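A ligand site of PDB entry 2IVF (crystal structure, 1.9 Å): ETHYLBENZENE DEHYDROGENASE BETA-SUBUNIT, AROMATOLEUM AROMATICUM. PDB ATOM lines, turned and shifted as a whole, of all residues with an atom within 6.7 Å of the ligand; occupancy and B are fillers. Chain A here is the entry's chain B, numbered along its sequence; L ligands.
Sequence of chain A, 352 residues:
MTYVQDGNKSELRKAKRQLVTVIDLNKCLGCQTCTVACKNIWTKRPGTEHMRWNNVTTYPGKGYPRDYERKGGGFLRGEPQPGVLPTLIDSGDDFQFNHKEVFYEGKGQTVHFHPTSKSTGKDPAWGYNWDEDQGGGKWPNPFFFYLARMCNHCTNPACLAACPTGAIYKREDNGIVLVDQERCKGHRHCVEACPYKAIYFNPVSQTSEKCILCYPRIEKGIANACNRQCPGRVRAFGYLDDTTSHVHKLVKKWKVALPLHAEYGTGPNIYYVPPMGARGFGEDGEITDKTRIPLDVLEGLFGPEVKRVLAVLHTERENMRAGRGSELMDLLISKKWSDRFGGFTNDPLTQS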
ATOM      1  N   MET A 150      21.233  -5.657  27.592  1.00  0.00           N
ATOM      2  CA  MET A 150      20.077  -6.101  28.334  1.00  0.00           C
ATOM      3  C   MET A 150      19.821  -7.531  27.900  1.00  0.00           C
ATOM      4  O   MET A 150      20.635  -8.114  27.164  1.00  0.00           O
ATOM      5  CB  MET A 150      18.831  -5.252  27.998  1.00  0.00           C
ATOM      6  CG  MET A 150      19.005  -3.784  27.990  1.00  0.00           C
ATOM      7  SD  MET A 150      19.564  -3.056  26.424  1.00  0.00           S
ATOM      8  CE  MET A 150      17.992  -3.108  25.509  1.00  0.00           C
ATOM      9  N   CYS A 151      18.679  -8.104  28.269  1.00  0.00           N
ATOM     10  CA  CYS A 151      18.320  -9.410  27.735  1.00  0.00           C
ATOM     11  C   CYS A 151      18.049  -9.214  26.256  1.00  0.00           C
ATOM     12  O   CYS A 151      17.444  -8.231  25.852  1.00  0.00           O
ATOM     13  CB  CYS A 151      17.119 -10.025  28.426  1.00  0.00           C
ATOM     14  SG  CYS A 151      16.325 -11.359  27.512  1.00  0.00           S
ATOM     15  N   ASN A 152      18.512 -10.174  25.458  1.00  0.00           N
ATOM     16  CA  ASN A 152      18.398 -10.099  24.015  1.00  0.00           C
ATOM     17  C   ASN A 152      17.076 -10.612  23.472  1.00  0.00           C
ATOM     18  O   ASN A 152      16.867 -10.565  22.278  1.00  0.00           O
ATOM     19  CB  ASN A 152      19.601 -10.837  23.378  1.00  0.00           C
ATOM     20  CG  ASN A 152      20.904 -10.243  23.786  1.00  0.00           C
ATOM     21  OD1 ASN A 152      21.199  -9.091  23.428  1.00  0.00           O
ATOM     22  ND2 ASN A 152      21.649 -10.947  24.628  1.00  0.00           N
ATOM     23  N   HIS A 153      16.189 -11.138  24.329  1.00  0.00           N
ATOM     24  CA  HIS A 153      14.923 -11.708  23.882  1.00  0.00           C
ATOM     25  C   HIS A 153      15.081 -12.561  22.671  1.00  0.00           C
ATOM     26  O   HIS A 153      14.386 -12.429  21.655  1.00  0.00           O
ATOM     27  CB  HIS A 153      13.859 -10.624  23.764  1.00  0.00           C
ATOM     28  CG  HIS A 153      13.640  -9.926  25.042  1.00  0.00           C
ATOM     29  ND1 HIS A 153      12.865 -10.455  26.056  1.00  0.00           N
ATOM     30  CD2 HIS A 153      14.202  -8.801  25.555  1.00  0.00           C
ATOM     31  CE1 HIS A 153      12.901  -9.653  27.102  1.00  0.00           C
ATOM     32  NE2 HIS A 153      13.703  -8.637  26.816  1.00  0.00           N
ATOM     33  N   CYS A 154      16.004 -13.503  22.855  1.00  0.00           N
ATOM     34  CA  CYS A 154      16.471 -14.367  21.814  1.00  0.00           C
ATOM     35  C   CYS A 154      15.380 -15.117  21.085  1.00  0.00           C
ATOM     36  O   CYS A 154      14.313 -15.438  21.628  1.00  0.00           O
ATOM     37  CB  CYS A 154      17.470 -15.356  22.430  1.00  0.00           C
ATOM     38  SG  CYS A 154      18.828 -14.520  23.253  1.00  0.00           S
ATOM     39  N   THR A 155      15.672 -15.414  19.826  1.00  0.00           N
ATOM     40  CA  THR A 155      14.785 -16.260  19.009  1.00  0.00           C
ATOM     41  C   THR A 155      14.911 -17.721  19.408  1.00  0.00           C
ATOM     42  O   THR A 155      13.949 -18.475  19.348  1.00  0.00           O
ATOM     43  CB  THR A 155      15.197 -16.114  17.533  1.00  0.00           C
ATOM     44  OG1 THR A 155      15.054 -14.744  17.154  1.00  0.00           O
ATOM     45  CG2 THR A 155      14.354 -16.987  16.631  1.00  0.00           C
ATOM     46  N   ASN A 156      16.118 -18.121  19.814  1.00  0.00           N
ATOM     47  CA  ASN A 156      16.328 -19.473  20.312  1.00  0.00           C
ATOM     48  C   ASN A 156      16.895 -19.417  21.724  1.00  0.00           C
ATOM     49  O   ASN A 156      18.071 -19.701  21.930  1.00  0.00           O
ATOM     50  CB  ASN A 156      17.243 -20.239  19.405  1.00  0.00           C
ATOM     51  CG  ASN A 156      17.507 -21.640  19.896  1.00  0.00           C
ATOM     52  OD1 ASN A 156      16.589 -22.296  20.390  1.00  0.00           O
ATOM     53  ND2 ASN A 156      18.786 -22.092  19.828  1.00  0.00           N
ATOM     54  N   PRO A 157      16.058 -19.011  22.702  1.00  0.00           N
ATOM     55  CA  PRO A 157      16.539 -18.704  24.049  1.00  0.00           C
ATOM     56  C   PRO A 157      17.023 -19.931  24.797  1.00  0.00           C
ATOM     57  O   PRO A 157      16.309 -20.948  24.865  1.00  0.00           O
ATOM     58  CB  PRO A 157      15.352 -18.037  24.749  1.00  0.00           C
ATOM     59  CG  PRO A 157      14.185 -18.287  23.907  1.00  0.00           C
ATOM     60  CD  PRO A 157      14.619 -18.772  22.549  1.00  0.00           C
ATOM     61  N   ALA A 158      18.240 -19.850  25.306  1.00  0.00           N
ATOM     62  CA  ALA A 158      18.837 -20.981  25.991  1.00  0.00           C
ATOM     63  C   ALA A 158      18.236 -21.115  27.391  1.00  0.00           C
ATOM     64  O   ALA A 158      18.064 -22.210  27.877  1.00  0.00           O
ATOM     65  CB  ALA A 158      20.318 -20.843  26.056  1.00  0.00           C
ATOM     66  N   CYS A 159      17.892 -19.992  27.985  1.00  0.00           N
ATOM     67  CA  CYS A 159      17.251 -19.944  29.283  1.00  0.00           C
ATOM     68  C   CYS A 159      15.979 -20.775  29.295  1.00  0.00           C
ATOM     69  O   CYS A 159      15.768 -21.604  30.180  1.00  0.00           O
ATOM     70  CB  CYS A 159      16.965 -18.496  29.615  1.00  0.00           C
ATOM     71  SG  CYS A 159      15.926 -17.587  28.426  1.00  0.00           S
ATOM     72  N   LEU A 160      15.121 -20.537  28.326  1.00  0.00           N
ATOM     73  CA  LEU A 160      13.871 -21.287  28.184  1.00  0.00           C
ATOM     74  C   LEU A 160      14.059 -22.785  28.090  1.00  0.00           C
ATOM     75  O   LEU A 160      13.322 -23.567  28.716  1.00  0.00           O
ATOM     76  CB  LEU A 160      13.143 -20.770  26.964  1.00  0.00           C
ATOM     77  CG  LEU A 160      11.726 -21.268  26.632  1.00  0.00           C
ATOM     78  CD1 LEU A 160      11.061 -20.159  25.746  1.00  0.00           C
ATOM     79  CD2 LEU A 160      11.725 -22.572  25.926  1.00  0.00           C
ATOM     80  N   ILE A 168       9.887 -20.455  32.026  1.00  0.00           N
ATOM     81  CA  ILE A 168      10.288 -19.411  31.088  1.00  0.00           C
ATOM     82  C   ILE A 168       9.543 -19.596  29.774  1.00  0.00           C
ATOM     83  O   ILE A 168       9.430 -20.712  29.232  1.00  0.00           O
ATOM     84  CB  ILE A 168      11.796 -19.418  30.816  1.00  0.00           C
ATOM     85  CG1 ILE A 168      12.540 -19.088  32.109  1.00  0.00           C
ATOM     86  CG2 ILE A 168      12.199 -18.444  29.645  1.00  0.00           C
ATOM     87  CD1 ILE A 168      14.052 -19.100  31.981  1.00  0.00           C
ATOM     88  N   LYS A 170       8.332 -17.459  25.859  1.00  0.00           N
ATOM     89  CA  LYS A 170       8.590 -16.390  24.906  1.00  0.00           C
ATOM     90  C   LYS A 170       7.235 -16.014  24.348  1.00  0.00           C
ATOM     91  O   LYS A 170       6.554 -16.870  23.789  1.00  0.00           O
ATOM     92  CB  LYS A 170       9.473 -16.872  23.777  1.00  0.00           C
ATOM     93  CG  LYS A 170       9.943 -15.774  22.825  1.00  0.00           C
ATOM     94  CD  LYS A 170      10.994 -16.332  21.856  1.00  0.00           C
ATOM     95  CE  LYS A 170      11.358 -15.290  20.750  1.00  0.00           C
ATOM     96  NZ  LYS A 170      12.038 -14.065  21.293  1.00  0.00           N
ATOM     97  N   VAL A 177      10.736 -12.572  26.238  1.00  0.00           N
ATOM     98  CA  VAL A 177      11.039 -13.776  27.001  1.00  0.00           C
ATOM     99  C   VAL A 177      10.857 -13.422  28.464  1.00  0.00           C
ATOM    100  O   VAL A 177      11.356 -12.424  28.943  1.00  0.00           O
ATOM    101  CB  VAL A 177      12.460 -14.288  26.728  1.00  0.00           C
ATOM    102  CG1 VAL A 177      12.795 -15.511  27.637  1.00  0.00           C
ATOM    103  CG2 VAL A 177      12.592 -14.618  25.249  1.00  0.00           C
ATOM    104  N   CYS A 190      18.544 -21.924  34.106  1.00  0.00           N
ATOM    105  CA  CYS A 190      18.396 -20.856  33.109  1.00  0.00           C
ATOM    106  C   CYS A 190      19.511 -19.885  33.196  1.00  0.00           C
ATOM    107  O   CYS A 190      20.006 -19.407  32.186  1.00  0.00           O
ATOM    108  CB  CYS A 190      17.078 -20.108  33.321  1.00  0.00           C
ATOM    109  SG  CYS A 190      16.906 -19.388  35.012  1.00  0.00           S
ATOM    110  N   ALA A 193      22.544 -21.484  31.697  1.00  0.00           N
ATOM    111  CA  ALA A 193      22.299 -21.656  30.280  1.00  0.00           C
ATOM    112  C   ALA A 193      22.359 -20.380  29.441  1.00  0.00           C
ATOM    113  O   ALA A 193      22.694 -20.446  28.280  1.00  0.00           O
ATOM    114  CB  ALA A 193      20.941 -22.333  30.076  1.00  0.00           C
ATOM    115  N   CYS A 194      21.969 -19.258  29.995  1.00  0.00           N
ATOM    116  CA  CYS A 194      21.981 -18.020  29.258  1.00  0.00           C
ATOM    117  C   CYS A 194      23.430 -17.577  29.104  1.00  0.00           C
ATOM    118  O   CYS A 194      24.064 -17.244  30.084  1.00  0.00           O
ATOM    119  CB  CYS A 194      21.192 -16.915  29.951  1.00  0.00           C
ATOM    120  SG  CYS A 194      21.596 -15.289  29.236  1.00  0.00           S
ATOM    121  N   PRO A 195      23.951 -17.572  27.860  1.00  0.00           N
ATOM    122  CA  PRO A 195      25.360 -17.279  27.674  1.00  0.00           C
ATOM    123  C   PRO A 195      25.647 -15.823  27.844  1.00  0.00           C
ATOM    124  O   PRO A 195      26.806 -15.429  27.820  1.00  0.00           O
ATOM    125  CB  PRO A 195      25.590 -17.688  26.237  1.00  0.00           C
ATOM    126  CG  PRO A 195      24.314 -17.402  25.592  1.00  0.00           C
ATOM    127  CD  PRO A 195      23.270 -17.787  26.579  1.00  0.00           C
ATOM    128  N   TYR A 196      24.603 -15.015  27.971  1.00  0.00           N
ATOM    129  CA  TYR A 196      24.758 -13.576  28.276  1.00  0.00           C
ATOM    130  C   TYR A 196      24.686 -13.230  29.772  1.00  0.00           C
ATOM    131  O   TYR A 196      24.869 -12.044  30.188  1.00  0.00           O
ATOM    132  CB  TYR A 196      23.686 -12.815  27.529  1.00  0.00           C
ATOM    133  CG  TYR A 196      23.796 -12.966  26.057  1.00  0.00           C
ATOM    134  CD1 TYR A 196      24.635 -12.141  25.304  1.00  0.00           C
ATOM    135  CD2 TYR A 196      23.054 -13.919  25.413  1.00  0.00           C
ATOM    136  CE1 TYR A 196      24.776 -12.336  23.904  1.00  0.00           C
ATOM    137  CE2 TYR A 196      23.145 -14.101  24.016  1.00  0.00           C
ATOM    138  CZ  TYR A 196      24.005 -13.298  23.257  1.00  0.00           C
ATOM    139  OH  TYR A 196      24.051 -13.544  21.897  1.00  0.00           O
ATOM    140  N   LYS A 197      24.342 -14.244  30.565  1.00  0.00           N
ATOM    141  CA  LYS A 197      24.037 -14.088  31.993  1.00  0.00           C
ATOM    142  C   LYS A 197      23.074 -12.944  32.246  1.00  0.00           C
ATOM    143  O   LYS A 197      23.329 -12.082  33.097  1.00  0.00           O
ATOM    144  CB  LYS A 197      25.332 -13.982  32.814  1.00  0.00           C
ATOM    145  CG  LYS A 197      26.186 -15.264  32.714  1.00  0.00           C
ATOM    146  CD  LYS A 197      25.472 -16.436  33.391  1.00  0.00           C
ATOM    147  CE  LYS A 197      26.086 -17.806  33.179  1.00  0.00           C
ATOM    148  NZ  LYS A 197      25.999 -18.368  31.800  1.00  0.00           N
ATOM    149  N   ALA A 198      22.005 -12.938  31.449  1.00  0.00           N
ATOM    150  CA  ALA A 198      20.968 -11.904  31.475  1.00  0.00           C
ATOM    151  C   ALA A 198      19.734 -12.348  32.310  1.00  0.00           C
ATOM    152  O   ALA A 198      18.667 -11.742  32.233  1.00  0.00           O
ATOM    153  CB  ALA A 198      20.565 -11.539  30.041  1.00  0.00           C
ATOM    154  N   ILE A 199      19.877 -13.416  33.081  1.00  0.00           N
ATOM    155  CA  ILE A 199      18.874 -13.788  34.069  1.00  0.00           C
ATOM    156  C   ILE A 199      19.591 -13.801  35.398  1.00  0.00           C
ATOM    157  O   ILE A 199      20.744 -14.260  35.473  1.00  0.00           O
ATOM    158  CB  ILE A 199      18.261 -15.185  33.829  1.00  0.00           C
ATOM    159  CG1 ILE A 199      17.710 -15.349  32.427  1.00  0.00           C
ATOM    160  CG2 ILE A 199      17.157 -15.472  34.838  1.00  0.00           C
ATOM    161  CD1 ILE A 199      16.761 -16.621  32.247  1.00  0.00           C
ATOM    162  N   LYS A 210      14.607 -11.055  35.248  1.00  0.00           N
ATOM    163  CA  LYS A 210      15.290 -10.612  34.065  1.00  0.00           C
ATOM    164  C   LYS A 210      14.529  -9.429  33.445  1.00  0.00           C
ATOM    165  O   LYS A 210      13.382  -9.140  33.780  1.00  0.00           O
ATOM    166  CB  LYS A 210      15.331 -11.777  33.048  1.00  0.00           C
ATOM    167  CG  LYS A 210      13.982 -12.154  32.491  1.00  0.00           C
ATOM    168  CD  LYS A 210      14.051 -13.255  31.461  1.00  0.00           C
ATOM    169  CE  LYS A 210      14.656 -12.848  30.150  1.00  0.00           C
ATOM    170  NZ  LYS A 210      14.015 -11.621  29.586  1.00  0.00           N
ATOM    171  N   CYS A 211      15.170  -8.821  32.469  1.00  0.00           N
ATOM    172  CA  CYS A 211      14.526  -7.807  31.664  1.00  0.00           C
ATOM    173  C   CYS A 211      13.200  -8.316  31.143  1.00  0.00           C
ATOM    174  O   CYS A 211      13.122  -9.395  30.575  1.00  0.00           O
ATOM    175  CB  CYS A 211      15.462  -7.421  30.538  1.00  0.00           C
ATOM    176  SG  CYS A 211      14.816  -6.424  29.226  1.00  0.00           S
ATOM    177  N   THR A 266      21.952 -18.404  20.165  1.00  0.00           N
ATOM    178  CA  THR A 266      20.622 -18.082  20.660  1.00  0.00           C
ATOM    179  C   THR A 266      19.815 -17.149  19.756  1.00  0.00           C
ATOM    180  O   THR A 266      18.624 -17.000  19.989  1.00  0.00           O
ATOM    181  CB  THR A 266      20.698 -17.435  22.048  1.00  0.00           C
ATOM    182  OG1 THR A 266      21.253 -16.116  21.977  1.00  0.00           O
ATOM    183  CG2 THR A 266      21.533 -18.301  23.011  1.00  0.00           C
ATOM    184  N   PRO A 268      20.166 -13.653  19.179  1.00  0.00           N
ATOM    185  CA  PRO A 268      19.827 -12.498  19.980  1.00  0.00           C
ATOM    186  C   PRO A 268      19.153 -11.403  19.167  1.00  0.00           C
ATOM    187  O   PRO A 268      19.418 -11.290  17.973  1.00  0.00           O
ATOM    188  CB  PRO A 268      21.184 -11.985  20.441  1.00  0.00           C
ATOM    189  CG  PRO A 268      22.074 -12.457  19.363  1.00  0.00           C
ATOM    190  CD  PRO A 268      21.614 -13.770  19.018  1.00  0.00           C
HETATM  191 FE1  LIG L   1      19.665 -14.971  27.940  1.00  0.00          FE
HETATM  192 FE2  LIG L   1      17.266 -16.008  27.620  1.00  0.00          FE
HETATM  193 FE3  LIG L   1      18.541 -14.842  25.491  1.00  0.00          FE
HETATM  194 FE4  LIG L   1      17.615 -13.255  27.530  1.00  0.00          FE
HETATM  195  S1  LIG L   1      16.356 -14.545  26.084  1.00  0.00           S
HETATM  196  S2  LIG L   1      19.701 -13.189  26.542  1.00  0.00           S
HETATM  197  S3  LIG L   1      17.881 -14.640  29.313  1.00  0.00           S
HETATM  198  S4  LIG L   1      19.167 -16.770  26.581  1.00  0.00           S
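FE1 of the ligand is bound by SG of Cys 194, at 2.3 Å.
The backbone NH (N) of Ala 158 sits close to a sulfur (S4) of the ligand, at 3.5 Å.
SG of Cys 154 binds FE3 of the ligand (2.3 Å).
The backbone NH of Cys 154 lies close to a sulfur (S1) of the ligand (3.4 Å).
FE4 of the ligand is bound by SG of Cys 151 (2.3 Å).
FE2 of the ligand is bound by SG of Cys 159 (2.2 Å).
N of Asn 152 sits close to S2 of the ligand, 3.4 Å away.
N of Cys 159 sits close to S4 of the ligand.
A sulfur (S2) of the ligand lies close to the side-chain amide nitrogen (ND2) of Asn 152, at 3.5 Å.
SG of Cys 194 sits close to N of Tyr 196 (3.3 Å).
SG of Cys 151 sits close to N of His 153 (3.2 Å).
The side-chain sulfur of Cys 194 lies close to the backbone NH of Ala 198 (3.3 Å).
The backbone carbonyl oxygen (O) of Cys 154 lies within hydrogen-bond range of the side-chain amino group (NZ) of Lys 170 (2.7 Å).
N of Val 177 lies within hydrogen-bond range of ND1 of His 153.
The backbone carbonyl oxygen of Cys 194 sits at hydrogen-bond distance from the side-chain amino group of Lys 197 (2.8 Å).
The side-chain sulfur of Cys 211 sits close to a ring nitrogen (NE2) of His 153 (3.5 Å).
The side-chain sulfur (SG) of Cys 154 lies close to the side-chain hydroxyl (OG1) of Thr 266 (3.2 Å).
Merely in contact with the ligand: Ile 199 (3.2 Å), Tyr 196 (3.6 Å), Lys 210 (3.8 Å), His 153 (3.8 Å), Val 177 (3.9 Å), Pro 157 (3.9 Å) and Ala 198 (3.96 Å).
Hydrophobic or aromatic side chains within 4 Å of the ligand: Pro 157, Val 177, Tyr 196, Ala 198 and Ile 199.
Of the 26 residues printed, 13 come within 4 Å of the ligand.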
